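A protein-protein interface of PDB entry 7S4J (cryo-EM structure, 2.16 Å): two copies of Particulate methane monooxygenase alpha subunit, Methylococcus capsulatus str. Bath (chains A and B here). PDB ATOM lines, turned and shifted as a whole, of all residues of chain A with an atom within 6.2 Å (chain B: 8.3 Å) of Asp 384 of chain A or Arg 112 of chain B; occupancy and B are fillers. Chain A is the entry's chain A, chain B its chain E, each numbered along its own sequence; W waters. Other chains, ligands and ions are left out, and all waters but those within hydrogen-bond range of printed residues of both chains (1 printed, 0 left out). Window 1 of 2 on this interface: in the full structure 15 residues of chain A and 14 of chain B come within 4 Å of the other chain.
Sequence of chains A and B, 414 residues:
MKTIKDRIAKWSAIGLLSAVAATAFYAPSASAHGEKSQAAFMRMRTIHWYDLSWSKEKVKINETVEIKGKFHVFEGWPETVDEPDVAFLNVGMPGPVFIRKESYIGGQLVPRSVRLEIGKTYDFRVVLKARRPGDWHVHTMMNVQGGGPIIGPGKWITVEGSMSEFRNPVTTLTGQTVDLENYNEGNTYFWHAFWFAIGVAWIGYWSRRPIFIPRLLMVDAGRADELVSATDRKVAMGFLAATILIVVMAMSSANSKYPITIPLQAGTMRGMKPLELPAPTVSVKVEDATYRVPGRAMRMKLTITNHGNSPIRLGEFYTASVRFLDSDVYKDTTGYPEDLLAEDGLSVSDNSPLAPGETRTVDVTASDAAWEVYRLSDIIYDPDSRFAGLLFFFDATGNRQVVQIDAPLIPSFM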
ATOM      1  N   PHE A  41      -1.697  34.404 -30.994  1.00  0.00           N
ATOM      2  CA  PHE A  41      -1.216  33.028 -31.026  1.00  0.00           C
ATOM      3  C   PHE A  41      -2.340  32.061 -31.373  1.00  0.00           C
ATOM      4  O   PHE A  41      -2.115  31.050 -32.045  1.00  0.00           O
ATOM      5  CB  PHE A  41      -0.558  32.662 -29.694  1.00  0.00           C
ATOM      6  CG  PHE A  41      -1.523  32.278 -28.608  1.00  0.00           C
ATOM      7  CD1 PHE A  41      -2.162  33.244 -27.856  1.00  0.00           C
ATOM      8  CD2 PHE A  41      -1.773  30.947 -28.328  1.00  0.00           C
ATOM      9  CE1 PHE A  41      -3.039  32.895 -26.854  1.00  0.00           C
ATOM     10  CE2 PHE A  41      -2.653  30.590 -27.329  1.00  0.00           C
ATOM     11  CZ  PHE A  41      -3.285  31.565 -26.589  1.00  0.00           C
ATOM     12  N   ARG A  45      -2.531  29.501 -34.475  1.00  0.00           N
ATOM     13  CA  ARG A  45      -2.723  28.064 -34.362  1.00  0.00           C
ATOM     14  C   ARG A  45      -4.173  27.728 -34.034  1.00  0.00           C
ATOM     15  O   ARG A  45      -4.485  27.286 -32.935  1.00  0.00           O
ATOM     16  CB  ARG A  45      -1.807  27.505 -33.269  1.00  0.00           C
ATOM     17  CG  ARG A  45      -0.524  28.257 -32.978  1.00  0.00           C
ATOM     18  CD  ARG A  45      -0.185  28.164 -31.499  1.00  0.00           C
ATOM     19  NE  ARG A  45       0.348  26.859 -31.125  1.00  0.00           N
ATOM     20  CZ  ARG A  45       1.581  26.435 -31.356  1.00  0.00           C
ATOM     21  NH1 ARG A  45       2.461  27.178 -32.001  1.00  0.00           N
ATOM     22  NH2 ARG A  45       1.934  25.225 -30.939  1.00  0.00           N
ATOM     23  N   PRO A  78      -4.978  24.690 -29.494  1.00  0.00           N
ATOM     24  CA  PRO A  78      -4.814  25.200 -28.126  1.00  0.00           C
ATOM     25  C   PRO A  78      -5.792  24.549 -27.159  1.00  0.00           C
ATOM     26  O   PRO A  78      -6.938  24.263 -27.506  1.00  0.00           O
ATOM     27  CB  PRO A  78      -5.072  26.703 -28.272  1.00  0.00           C
ATOM     28  CG  PRO A  78      -5.805  26.850 -29.555  1.00  0.00           C
ATOM     29  CD  PRO A  78      -5.346  25.750 -30.442  1.00  0.00           C
ATOM     30  N   ILE A 379       1.127  39.491 -30.010  1.00  0.00           N
ATOM     31  CA  ILE A 379       1.449  38.221 -29.369  1.00  0.00           C
ATOM     32  C   ILE A 379       2.247  38.417 -28.088  1.00  0.00           C
ATOM     33  O   ILE A 379       2.215  37.545 -27.209  1.00  0.00           O
ATOM     34  CB  ILE A 379       2.201  37.303 -30.357  1.00  0.00           C
ATOM     35  CG1 ILE A 379       2.399  35.905 -29.767  1.00  0.00           C
ATOM     36  CG2 ILE A 379       3.530  37.914 -30.752  1.00  0.00           C
ATOM     37  CD1 ILE A 379       2.338  34.799 -30.782  1.00  0.00           C
ATOM     38  N   ASP A 382       0.162  37.922 -25.194  1.00  0.00           N
ATOM     39  CA  ASP A 382      -0.483  36.633 -25.036  1.00  0.00           C
ATOM     40  C   ASP A 382       0.223  35.779 -23.986  1.00  0.00           C
ATOM     41  O   ASP A 382       1.439  35.866 -23.817  1.00  0.00           O
ATOM     42  CB  ASP A 382      -0.511  35.893 -26.367  1.00  0.00           C
ATOM     43  CG  ASP A 382      -1.508  36.490 -27.341  1.00  0.00           C
ATOM     44  OD1 ASP A 382      -2.497  37.098 -26.881  1.00  0.00           O
ATOM     45  OD2 ASP A 382      -1.307  36.348 -28.564  1.00  0.00           O
ATOM     46  N   PRO A 383      -0.526  34.936 -23.273  1.00  0.00           N
ATOM     47  CA  PRO A 383       0.086  34.002 -22.323  1.00  0.00           C
ATOM     48  C   PRO A 383       0.704  32.770 -22.964  1.00  0.00           C
ATOM     49  O   PRO A 383       1.072  31.841 -22.242  1.00  0.00           O
ATOM     50  CB  PRO A 383      -1.102  33.610 -21.436  1.00  0.00           C
ATOM     51  CG  PRO A 383      -2.266  33.698 -22.336  1.00  0.00           C
ATOM     52  CD  PRO A 383      -1.994  34.836 -23.277  1.00  0.00           C
ATOM     53  N   ASP A 384       0.822  32.728 -24.287  1.00  0.00           N
ATOM     54  CA  ASP A 384       1.400  31.574 -24.971  1.00  0.00           C
ATOM     55  C   ASP A 384       2.092  32.098 -26.225  1.00  0.00           C
ATOM     56  O   ASP A 384       1.456  32.249 -27.269  1.00  0.00           O
ATOM     57  CB  ASP A 384       0.326  30.549 -25.305  1.00  0.00           C
ATOM     58  CG  ASP A 384       0.900  29.198 -25.658  1.00  0.00           C
ATOM     59  OD1 ASP A 384       2.138  29.074 -25.742  1.00  0.00           O
ATOM     60  OD2 ASP A 384       0.108  28.254 -25.848  1.00  0.00           O
ATOM     61  N   SER A 385       3.392  32.364 -26.117  1.00  0.00           N
ATOM     62  CA  SER A 385       4.152  32.953 -27.220  1.00  0.00           C
ATOM     63  C   SER A 385       4.664  31.855 -28.150  1.00  0.00           C
ATOM     64  O   SER A 385       5.852  31.546 -28.225  1.00  0.00           O
ATOM     65  CB  SER A 385       5.291  33.805 -26.684  1.00  0.00           C
ATOM     66  OG  SER A 385       5.629  34.826 -27.603  1.00  0.00           O
ATOM     67  N   ARG A 386       3.723  31.267 -28.875  1.00  0.00           N
ATOM     68  CA  ARG A 386       4.023  30.266 -29.881  1.00  0.00           C
ATOM     69  C   ARG A 386       3.287  30.617 -31.162  1.00  0.00           C
ATOM     70  O   ARG A 386       2.165  31.126 -31.132  1.00  0.00           O
ATOM     71  CB  ARG A 386       3.632  28.861 -29.412  1.00  0.00           C
ATOM     72  CG  ARG A 386       4.617  28.241 -28.443  1.00  0.00           C
ATOM     73  CD  ARG A 386       4.248  26.808 -28.120  1.00  0.00           C
ATOM     74  NE  ARG A 386       2.968  26.708 -27.431  1.00  0.00           N
ATOM     75  CZ  ARG A 386       2.273  25.587 -27.309  1.00  0.00           C
ATOM     76  NH1 ARG A 386       2.696  24.452 -27.836  1.00  0.00           N
ATOM     77  NH2 ARG A 386       1.124  25.607 -26.643  1.00  0.00           N
ATOM     78  N   PHE A 387       3.929  30.345 -32.289  1.00  0.00           N
ATOM     79  CA  PHE A 387       3.356  30.624 -33.592  1.00  0.00           C
ATOM     80  C   PHE A 387       3.231  29.334 -34.389  1.00  0.00           C
ATOM     81  O   PHE A 387       3.868  28.324 -34.085  1.00  0.00           O
ATOM     82  CB  PHE A 387       4.202  31.638 -34.370  1.00  0.00           C
ATOM     83  CG  PHE A 387       5.310  31.016 -35.165  1.00  0.00           C
ATOM     84  CD1 PHE A 387       6.501  30.667 -34.558  1.00  0.00           C
ATOM     85  CD2 PHE A 387       5.161  30.778 -36.520  1.00  0.00           C
ATOM     86  CE1 PHE A 387       7.520  30.092 -35.285  1.00  0.00           C
ATOM     87  CE2 PHE A 387       6.173  30.197 -37.249  1.00  0.00           C
ATOM     88  CZ  PHE A 387       7.357  29.859 -36.633  1.00  0.00           C
ATOM     89  N   VAL B  86      -4.012  15.924 -20.454  1.00  0.00           N
ATOM     90  CA  VAL B  86      -3.268  17.014 -19.839  1.00  0.00           C
ATOM     91  C   VAL B  86      -2.414  16.378 -18.750  1.00  0.00           C
ATOM     92  O   VAL B  86      -2.923  16.018 -17.684  1.00  0.00           O
ATOM     93  CB  VAL B  86      -4.182  18.100 -19.268  1.00  0.00           C
ATOM     94  CG1 VAL B  86      -3.364  19.185 -18.640  1.00  0.00           C
ATOM     95  CG2 VAL B  86      -5.077  18.674 -20.355  1.00  0.00           C
ATOM     96  N   ALA B  87      -1.122  16.225 -19.014  1.00  0.00           N
ATOM     97  CA  ALA B  87      -0.215  15.562 -18.094  1.00  0.00           C
ATOM     98  C   ALA B  87       1.029  16.410 -17.890  1.00  0.00           C
ATOM     99  O   ALA B  87       1.464  17.126 -18.792  1.00  0.00           O
ATOM    100  CB  ALA B  87       0.178  14.171 -18.600  1.00  0.00           C
ATOM    101  N   PHE B  88       1.601  16.322 -16.694  1.00  0.00           N
ATOM    102  CA  PHE B  88       2.786  17.085 -16.336  1.00  0.00           C
ATOM    103  C   PHE B  88       3.887  16.136 -15.894  1.00  0.00           C
ATOM    104  O   PHE B  88       3.665  15.280 -15.035  1.00  0.00           O
ATOM    105  CB  PHE B  88       2.478  18.092 -15.227  1.00  0.00           C
ATOM    106  CG  PHE B  88       3.647  18.947 -14.847  1.00  0.00           C
ATOM    107  CD1 PHE B  88       4.147  19.888 -15.725  1.00  0.00           C
ATOM    108  CD2 PHE B  88       4.254  18.804 -13.614  1.00  0.00           C
ATOM    109  CE1 PHE B  88       5.223  20.673 -15.381  1.00  0.00           C
ATOM    110  CE2 PHE B  88       5.330  19.587 -13.264  1.00  0.00           C
ATOM    111  CZ  PHE B  88       5.815  20.522 -14.149  1.00  0.00           C
ATOM    112  N   LEU B  89       5.072  16.295 -16.477  1.00  0.00           N
ATOM    113  CA  LEU B  89       6.240  15.503 -16.098  1.00  0.00           C
ATOM    114  C   LEU B  89       6.846  16.142 -14.856  1.00  0.00           C
ATOM    115  O   LEU B  89       7.528  17.163 -14.937  1.00  0.00           O
ATOM    116  CB  LEU B  89       7.247  15.431 -17.239  1.00  0.00           C
ATOM    117  CG  LEU B  89       8.535  14.665 -16.934  1.00  0.00           C
ATOM    118  CD1 LEU B  89       8.236  13.194 -16.701  1.00  0.00           C
ATOM    119  CD2 LEU B  89       9.553  14.837 -18.047  1.00  0.00           C
ATOM    120  N   ASN B  90       6.591  15.542 -13.705  1.00  0.00           N
ATOM    121  CA  ASN B  90       7.015  16.094 -12.433  1.00  0.00           C
ATOM    122  C   ASN B  90       8.154  15.263 -11.853  1.00  0.00           C
ATOM    123  O   ASN B  90       8.579  14.256 -12.418  1.00  0.00           O
ATOM    124  CB  ASN B  90       5.822  16.167 -11.478  1.00  0.00           C
ATOM    125  CG  ASN B  90       5.888  17.361 -10.558  1.00  0.00           C
ATOM    126  OD1 ASN B  90       6.829  18.146 -10.613  1.00  0.00           O
ATOM    127  ND2 ASN B  90       4.878  17.514  -9.718  1.00  0.00           N
ATOM    128  N   ARG B 100      14.470  21.716 -10.681  1.00  0.00           N
ATOM    129  CA  ARG B 100      14.332  21.172 -12.027  1.00  0.00           C
ATOM    130  C   ARG B 100      14.851  22.199 -13.021  1.00  0.00           C
ATOM    131  O   ARG B 100      14.189  23.195 -13.307  1.00  0.00           O
ATOM    132  CB  ARG B 100      12.878  20.817 -12.310  1.00  0.00           C
ATOM    133  CG  ARG B 100      12.662  20.120 -13.632  1.00  0.00           C
ATOM    134  CD  ARG B 100      11.189  19.996 -13.965  1.00  0.00           C
ATOM    135  NE  ARG B 100      10.370  20.930 -13.205  1.00  0.00           N
ATOM    136  CZ  ARG B 100       9.276  20.598 -12.538  1.00  0.00           C
ATOM    137  NH1 ARG B 100       8.842  19.351 -12.499  1.00  0.00           N
ATOM    138  NH2 ARG B 100       8.601  21.540 -11.889  1.00  0.00           N
ATOM    139  N   SER B 103      13.399  19.618 -18.383  1.00  0.00           N
ATOM    140  CA  SER B 103      12.682  18.357 -18.506  1.00  0.00           C
ATOM    141  C   SER B 103      12.202  18.229 -19.940  1.00  0.00           C
ATOM    142  O   SER B 103      11.690  19.193 -20.512  1.00  0.00           O
ATOM    143  CB  SER B 103      11.508  18.276 -17.525  1.00  0.00           C
ATOM    144  OG  SER B 103      10.672  19.410 -17.622  1.00  0.00           O
ATOM    145  N   ILE B 105      10.191  15.681 -22.936  1.00  0.00           N
ATOM    146  CA  ILE B 105       9.445  14.530 -23.425  1.00  0.00           C
ATOM    147  C   ILE B 105       9.752  14.418 -24.907  1.00  0.00           C
ATOM    148  O   ILE B 105       9.478  15.348 -25.675  1.00  0.00           O
ATOM    149  CB  ILE B 105       7.936  14.672 -23.187  1.00  0.00           C
ATOM    150  CG1 ILE B 105       7.627  14.787 -21.696  1.00  0.00           C
ATOM    151  CG2 ILE B 105       7.199  13.495 -23.799  1.00  0.00           C
ATOM    152  CD1 ILE B 105       7.828  13.520 -20.945  1.00  0.00           C
ATOM    153  N   LEU B 109      11.702  20.529 -24.648  1.00  0.00           N
ATOM    154  CA  LEU B 109      11.476  20.982 -23.284  1.00  0.00           C
ATOM    155  C   LEU B 109       9.986  21.098 -22.993  1.00  0.00           C
ATOM    156  O   LEU B 109       9.213  21.584 -23.819  1.00  0.00           O
ATOM    157  CB  LEU B 109      12.166  22.328 -23.063  1.00  0.00           C
ATOM    158  CG  LEU B 109      12.254  22.817 -21.621  1.00  0.00           C
ATOM    159  CD1 LEU B 109      13.599  22.446 -21.034  1.00  0.00           C
ATOM    160  CD2 LEU B 109      12.034  24.314 -21.554  1.00  0.00           C
ATOM    161  N   VAL B 110       9.585  20.657 -21.807  1.00  0.00           N
ATOM    162  CA  VAL B 110       8.168  20.618 -21.459  1.00  0.00           C
ATOM    163  C   VAL B 110       7.931  21.311 -20.121  1.00  0.00           C
ATOM    164  O   VAL B 110       7.599  20.651 -19.129  1.00  0.00           O
ATOM    165  CB  VAL B 110       7.644  19.172 -21.449  1.00  0.00           C
ATOM    166  CG1 VAL B 110       7.449  18.684 -22.869  1.00  0.00           C
ATOM    167  CG2 VAL B 110       8.604  18.249 -20.721  1.00  0.00           C
ATOM    168  N   PRO B 111       8.069  22.640 -20.046  1.00  0.00           N
ATOM    169  CA  PRO B 111       7.775  23.330 -18.785  1.00  0.00           C
ATOM    170  C   PRO B 111       6.294  23.429 -18.474  1.00  0.00           C
ATOM    171  O   PRO B 111       5.944  23.734 -17.328  1.00  0.00           O
ATOM    172  CB  PRO B 111       8.386  24.718 -19.000  1.00  0.00           C
ATOM    173  CG  PRO B 111       8.285  24.927 -20.457  1.00  0.00           C
ATOM    174  CD  PRO B 111       8.452  23.582 -21.108  1.00  0.00           C
ATOM    175  N   ARG B 112       5.421  23.191 -19.440  1.00  0.00           N
ATOM    176  CA  ARG B 112       3.986  23.190 -19.216  1.00  0.00           C
ATOM    177  C   ARG B 112       3.454  21.767 -19.296  1.00  0.00           C
ATOM    178  O   ARG B 112       4.184  20.816 -19.576  1.00  0.00           O
ATOM    179  CB  ARG B 112       3.275  24.095 -20.223  1.00  0.00           C
ATOM    180  CG  ARG B 112       4.175  25.089 -20.923  1.00  0.00           C
ATOM    181  CD  ARG B 112       3.555  26.467 -20.887  1.00  0.00           C
ATOM    182  NE  ARG B 112       4.069  27.329 -21.941  1.00  0.00           N
ATOM    183  CZ  ARG B 112       3.430  27.583 -23.073  1.00  0.00           C
ATOM    184  NH1 ARG B 112       2.248  27.051 -23.333  1.00  0.00           N
ATOM    185  NH2 ARG B 112       3.992  28.389 -23.967  1.00  0.00           N
ATOM    186  N   SER B 113       2.159  21.628 -19.040  1.00  0.00           N
ATOM    187  CA  SER B 113       1.513  20.336 -19.171  1.00  0.00           C
ATOM    188  C   SER B 113       1.488  19.909 -20.633  1.00  0.00           C
ATOM    189  O   SER B 113       1.533  20.736 -21.546  1.00  0.00           O
ATOM    190  CB  SER B 113       0.097  20.386 -18.606  1.00  0.00           C
ATOM    191  OG  SER B 113      -0.630  21.467 -19.155  1.00  0.00           O
ATOM    192  N   VAL B 114       1.437  18.602 -20.853  1.00  0.00           N
ATOM    193  CA  VAL B 114       1.504  18.042 -22.194  1.00  0.00           C
ATOM    194  C   VAL B 114       0.350  17.073 -22.391  1.00  0.00           C
ATOM    195  O   VAL B 114      -0.280  16.608 -21.440  1.00  0.00           O
ATOM    196  CB  VAL B 114       2.847  17.338 -22.466  1.00  0.00           C
ATOM    197  CG1 VAL B 114       3.992  18.278 -22.217  1.00  0.00           C
ATOM    198  CG2 VAL B 114       2.977  16.102 -21.601  1.00  0.00           C
ATOM    199  N   ARG B 115       0.081  16.770 -23.653  1.00  0.00           N
ATOM    200  CA  ARG B 115      -0.905  15.772 -24.027  1.00  0.00           C
ATOM    201  C   ARG B 115      -0.191  14.488 -24.422  1.00  0.00           C
ATOM    202  O   ARG B 115       0.681  14.501 -25.294  1.00  0.00           O
ATOM    203  CB  ARG B 115      -1.777  16.264 -25.179  1.00  0.00           C
ATOM    204  CG  ARG B 115      -2.547  15.161 -25.876  1.00  0.00           C
ATOM    205  CD  ARG B 115      -3.467  15.726 -26.932  1.00  0.00           C
ATOM    206  NE  ARG B 115      -4.789  16.012 -26.393  1.00  0.00           N
ATOM    207  CZ  ARG B 115      -5.861  15.264 -26.608  1.00  0.00           C
ATOM    208  NH1 ARG B 115      -5.806  14.179 -27.359  1.00  0.00           N
ATOM    209  NH2 ARG B 115      -7.016  15.616 -26.055  1.00  0.00           N
ATOM    210  N   ILE B 262       5.791  40.473 -19.518  1.00  0.00           N
ATOM    211  CA  ILE B 262       4.929  39.551 -20.248  1.00  0.00           C
ATOM    212  C   ILE B 262       4.026  38.854 -19.240  1.00  0.00           C
ATOM    213  O   ILE B 262       4.395  38.732 -18.066  1.00  0.00           O
ATOM    214  CB  ILE B 262       5.750  38.538 -21.061  1.00  0.00           C
ATOM    215  CG1 ILE B 262       6.707  37.769 -20.151  1.00  0.00           C
ATOM    216  CG2 ILE B 262       6.511  39.237 -22.172  1.00  0.00           C
ATOM    217  CD1 ILE B 262       7.056  36.394 -20.653  1.00  0.00           C
ATOM    218  N   PRO B 263       2.845  38.396 -19.638  1.00  0.00           N
ATOM    219  CA  PRO B 263       2.011  37.621 -18.714  1.00  0.00           C
ATOM    220  C   PRO B 263       2.626  36.259 -18.440  1.00  0.00           C
ATOM    221  O   PRO B 263       3.564  35.818 -19.103  1.00  0.00           O
ATOM    222  CB  PRO B 263       0.678  37.499 -19.454  1.00  0.00           C
ATOM    223  CG  PRO B 263       1.030  37.658 -20.885  1.00  0.00           C
ATOM    224  CD  PRO B 263       2.181  38.609 -20.934  1.00  0.00           C
ATOM    225  N   LEU B 264       2.088  35.598 -17.421  1.00  0.00           N
ATOM    226  CA  LEU B 264       2.496  34.233 -17.120  1.00  0.00           C
ATOM    227  C   LEU B 264       2.247  33.337 -18.325  1.00  0.00           C
ATOM    228  O   LEU B 264       1.168  33.361 -18.918  1.00  0.00           O
ATOM    229  CB  LEU B 264       1.734  33.714 -15.905  1.00  0.00           C
ATOM    230  CG  LEU B 264       2.020  34.405 -14.574  1.00  0.00           C
ATOM    231  CD1 LEU B 264       1.061  33.913 -13.513  1.00  0.00           C
ATOM    232  CD2 LEU B 264       3.450  34.165 -14.155  1.00  0.00           C
ATOM    233  N   GLN B 265       3.251  32.547 -18.686  1.00  0.00           N
ATOM    234  CA  GLN B 265       3.175  31.682 -19.855  1.00  0.00           C
ATOM    235  C   GLN B 265       2.581  30.341 -19.448  1.00  0.00           C
ATOM    236  O   GLN B 265       3.109  29.665 -18.560  1.00  0.00           O
ATOM    237  CB  GLN B 265       4.553  31.500 -20.482  1.00  0.00           C
ATOM    238  CG  GLN B 265       5.172  32.782 -21.003  1.00  0.00           C
ATOM    239  CD  GLN B 265       4.338  33.435 -22.085  1.00  0.00           C
ATOM    240  OE1 GLN B 265       4.361  33.015 -23.237  1.00  0.00           O
ATOM    241  NE2 GLN B 265       3.603  34.475 -21.721  1.00  0.00           N
ATOM    242  N   ALA B 266       1.489  29.955 -20.100  1.00  0.00           N
ATOM    243  CA  ALA B 266       0.767  28.748 -19.736  1.00  0.00           C
ATOM    244  C   ALA B 266       0.111  28.168 -20.976  1.00  0.00           C
ATOM    245  O   ALA B 266       0.000  28.826 -22.013  1.00  0.00           O
ATOM    246  CB  ALA B 266      -0.275  29.029 -18.650  1.00  0.00           C
ATOM    247  N   GLY B 267      -0.317  26.918 -20.861  1.00  0.00           N
ATOM    248  CA  GLY B 267      -0.976  26.249 -21.960  1.00  0.00           C
ATOM    249  C   GLY B 267      -0.426  24.867 -22.227  1.00  0.00           C
ATOM    250  O   GLY B 267       0.789  24.682 -22.324  1.00  0.00           O
ATOM    251  N   THR B 268      -1.316  23.887 -22.347  1.00  0.00           N
ATOM    252  CA  THR B 268      -0.899  22.521 -22.623  1.00  0.00           C
ATOM    253  C   THR B 268      -0.228  22.438 -23.987  1.00  0.00           C
ATOM    254  O   THR B 268      -0.653  23.082 -24.948  1.00  0.00           O
ATOM    255  CB  THR B 268      -2.104  21.583 -22.568  1.00  0.00           C
ATOM    256  OG1 THR B 268      -2.719  21.677 -21.280  1.00  0.00           O
ATOM    257  CG2 THR B 268      -1.686  20.142 -22.817  1.00  0.00           C
ATOM    258  N   MET B 269       0.833  21.647 -24.066  1.00  0.00           N
ATOM    259  CA  MET B 269       1.573  21.453 -25.302  1.00  0.00           C
ATOM    260  C   MET B 269       1.141  20.145 -25.949  1.00  0.00           C
ATOM    261  O   MET B 269       1.319  19.071 -25.368  1.00  0.00           O
ATOM    262  CB  MET B 269       3.075  21.451 -25.035  1.00  0.00           C
ATOM    263  CG  MET B 269       3.641  22.824 -24.738  1.00  0.00           C
ATOM    264  SD  MET B 269       5.118  22.738 -23.718  1.00  0.00           S
ATOM    265  CE  MET B 269       6.217  21.889 -24.834  1.00  0.00           C
ATOM    266  N   ARG B 270       0.567  20.214 -27.150  1.00  0.00           N
ATOM    267  CA  ARG B 270       0.240  18.969 -27.894  1.00  0.00           C
ATOM    268  C   ARG B 270       1.434  18.614 -28.789  1.00  0.00           C
ATOM    269  O   ARG B 270       2.449  19.335 -28.744  1.00  0.00           O
ATOM    270  CB  ARG B 270      -1.014  19.160 -28.749  1.00  0.00           C
ATOM    271  CG  ARG B 270      -2.315  19.235 -27.965  1.00  0.00           C
ATOM    272  CD  ARG B 270      -3.454  19.537 -28.917  1.00  0.00           C
ATOM    273  NE  ARG B 270      -4.562  18.592 -28.878  1.00  0.00           N
ATOM    274  CZ  ARG B 270      -4.799  17.666 -29.800  1.00  0.00           C
ATOM    275  NH1 ARG B 270      -3.996  17.541 -30.843  1.00  0.00           N
ATOM    276  NH2 ARG B 270      -5.835  16.857 -29.672  1.00  0.00           N
ATOM    277  N   MET B 272       3.435  15.895 -28.724  1.00  0.00           N
ATOM    278  CA  MET B 272       4.543  15.179 -28.104  1.00  0.00           C
ATOM    279  C   MET B 272       4.952  14.052 -29.042  1.00  0.00           C
ATOM    280  O   MET B 272       4.124  13.216 -29.410  1.00  0.00           O
ATOM    281  CB  MET B 272       4.143  14.631 -26.737  1.00  0.00           C
ATOM    282  CG  MET B 272       3.998  15.676 -25.649  1.00  0.00           C
ATOM    283  SD  MET B 272       5.479  16.667 -25.409  1.00  0.00           S
ATOM    284  CE  MET B 272       4.935  18.228 -26.090  1.00  0.00           C
HETATM  285  O   HOH W   1       0.408  22.523 -28.461  1.00  0.00           O
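The side-chain amide oxygen (OE1) of Gln 265 of chain B lies within hydrogen-bond range of the backbone NH (N) of Ser 385 of chain A, 3.1 Å away. The backbone carbonyl oxygen of Asp 382 of chain A lies within hydrogen-bond range of the side-chain amide nitrogen of Gln 265 of chain B (3.3 Å). OD1 of Asp 384 of chain A is in salt-bridge range of NH2 of Arg 112 of chain B (2.7 Å). O of Pro 383 of chain A is in hydrogen-bond range of N of Ala 266 of chain B (2.9 Å).
The backbone carbonyl oxygen (O) of Pro 263 of chain B is in hydrogen-bond range of the side-chain amide nitrogen (NE2) of Gln 265 of chain B (2.9 Å). OD2 of Asp 382 of chain A lies within hydrogen-bond range of N of Phe 41 of chain A (3.1 Å). The backbone carbonyl oxygen (O) of Met 269 of chain B lies within hydrogen-bond range of the backbone NH (N) of Arg 115 of chain B. The backbone carbonyl oxygen (O) of Ala 266 of chain B sits at hydrogen-bond distance from the guanidinium group (NH1) of Arg 112 of chain B, at 3.2 Å. The guanidinium group (NH1) of Arg 112 of chain B is in hydrogen-bond range of the backbone carbonyl oxygen (O) of Gly 267 of chain B, 3.0 Å away. The backbone NH (N) of Met 269 of chain B is in hydrogen-bond range of the backbone carbonyl oxygen (O) of Ser 113 of chain B, at 2.8 Å.
Among the printed residues, pairs that only touch across the chains: Pro 383 of chain A with Gln 265 of chain B (3.2 Å), Pro 383 of chain A with Leu 264 of chain B (3.4 Å), Asp 382 of chain A with Pro 263 of chain B (3.5 Å), Arg 386 of chain A with Thr 268 of chain B (3.5 Å), Arg 386 of chain A with Met 269 of chain B (3.6 Å), Asp 384 of chain A with Gln 265 of chain B (3.7 Å), Asp 384 of chain A with Ala 266 of chain B (3.7 Å), Arg 386 of chain A with Arg 112 of chain B (3.8 Å) and Pro 383 of chain A with Pro 263 of chain B (3.9 Å).
Printed residues of chain B within 4 Å of Asp 384 of chain A: Arg 112 (2.7 Å), Gln 265 (3.7 Å) and Ala 266 (3.7 Å). Arg 112 of chain B touches just these residues of chain A: Asp 384 and Arg 386. Of the printed residues of chain B, Ser 385 of chain A touches Gln 265 (3.1 Å). Of the printed residues of chain A, Ala 266 of chain B touches Pro 383 (2.9 Å) and Asp 384 (3.7 Å). Printed residues of chain A within 4 Å of Pro 263 of chain B: Asp 382 (3.5 Å) and Pro 383 (3.9 Å). Of the printed residues of chain B, Arg 386 of chain A touches Arg 112, Thr 268 and Met 269. The nearest residue of chain A that does not touch Arg 112 of chain B is Ser 385 of chain A (4.6 Å).
Printed residues of chain A that touch a printed residue of chain B: Asp 382, Pro 383, Asp 384, Ser 385 and Arg 386. Among the printed residues, 13 pairs touch across the chains.
No position is printed for both chains.
Water W1 lies within hydrogen-bond range of the backbone NH (N) of Arg 270 of chain B (2.7 Å) and the guanidinium group (NH1) of Arg 386 of chain A (3.1 Å).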
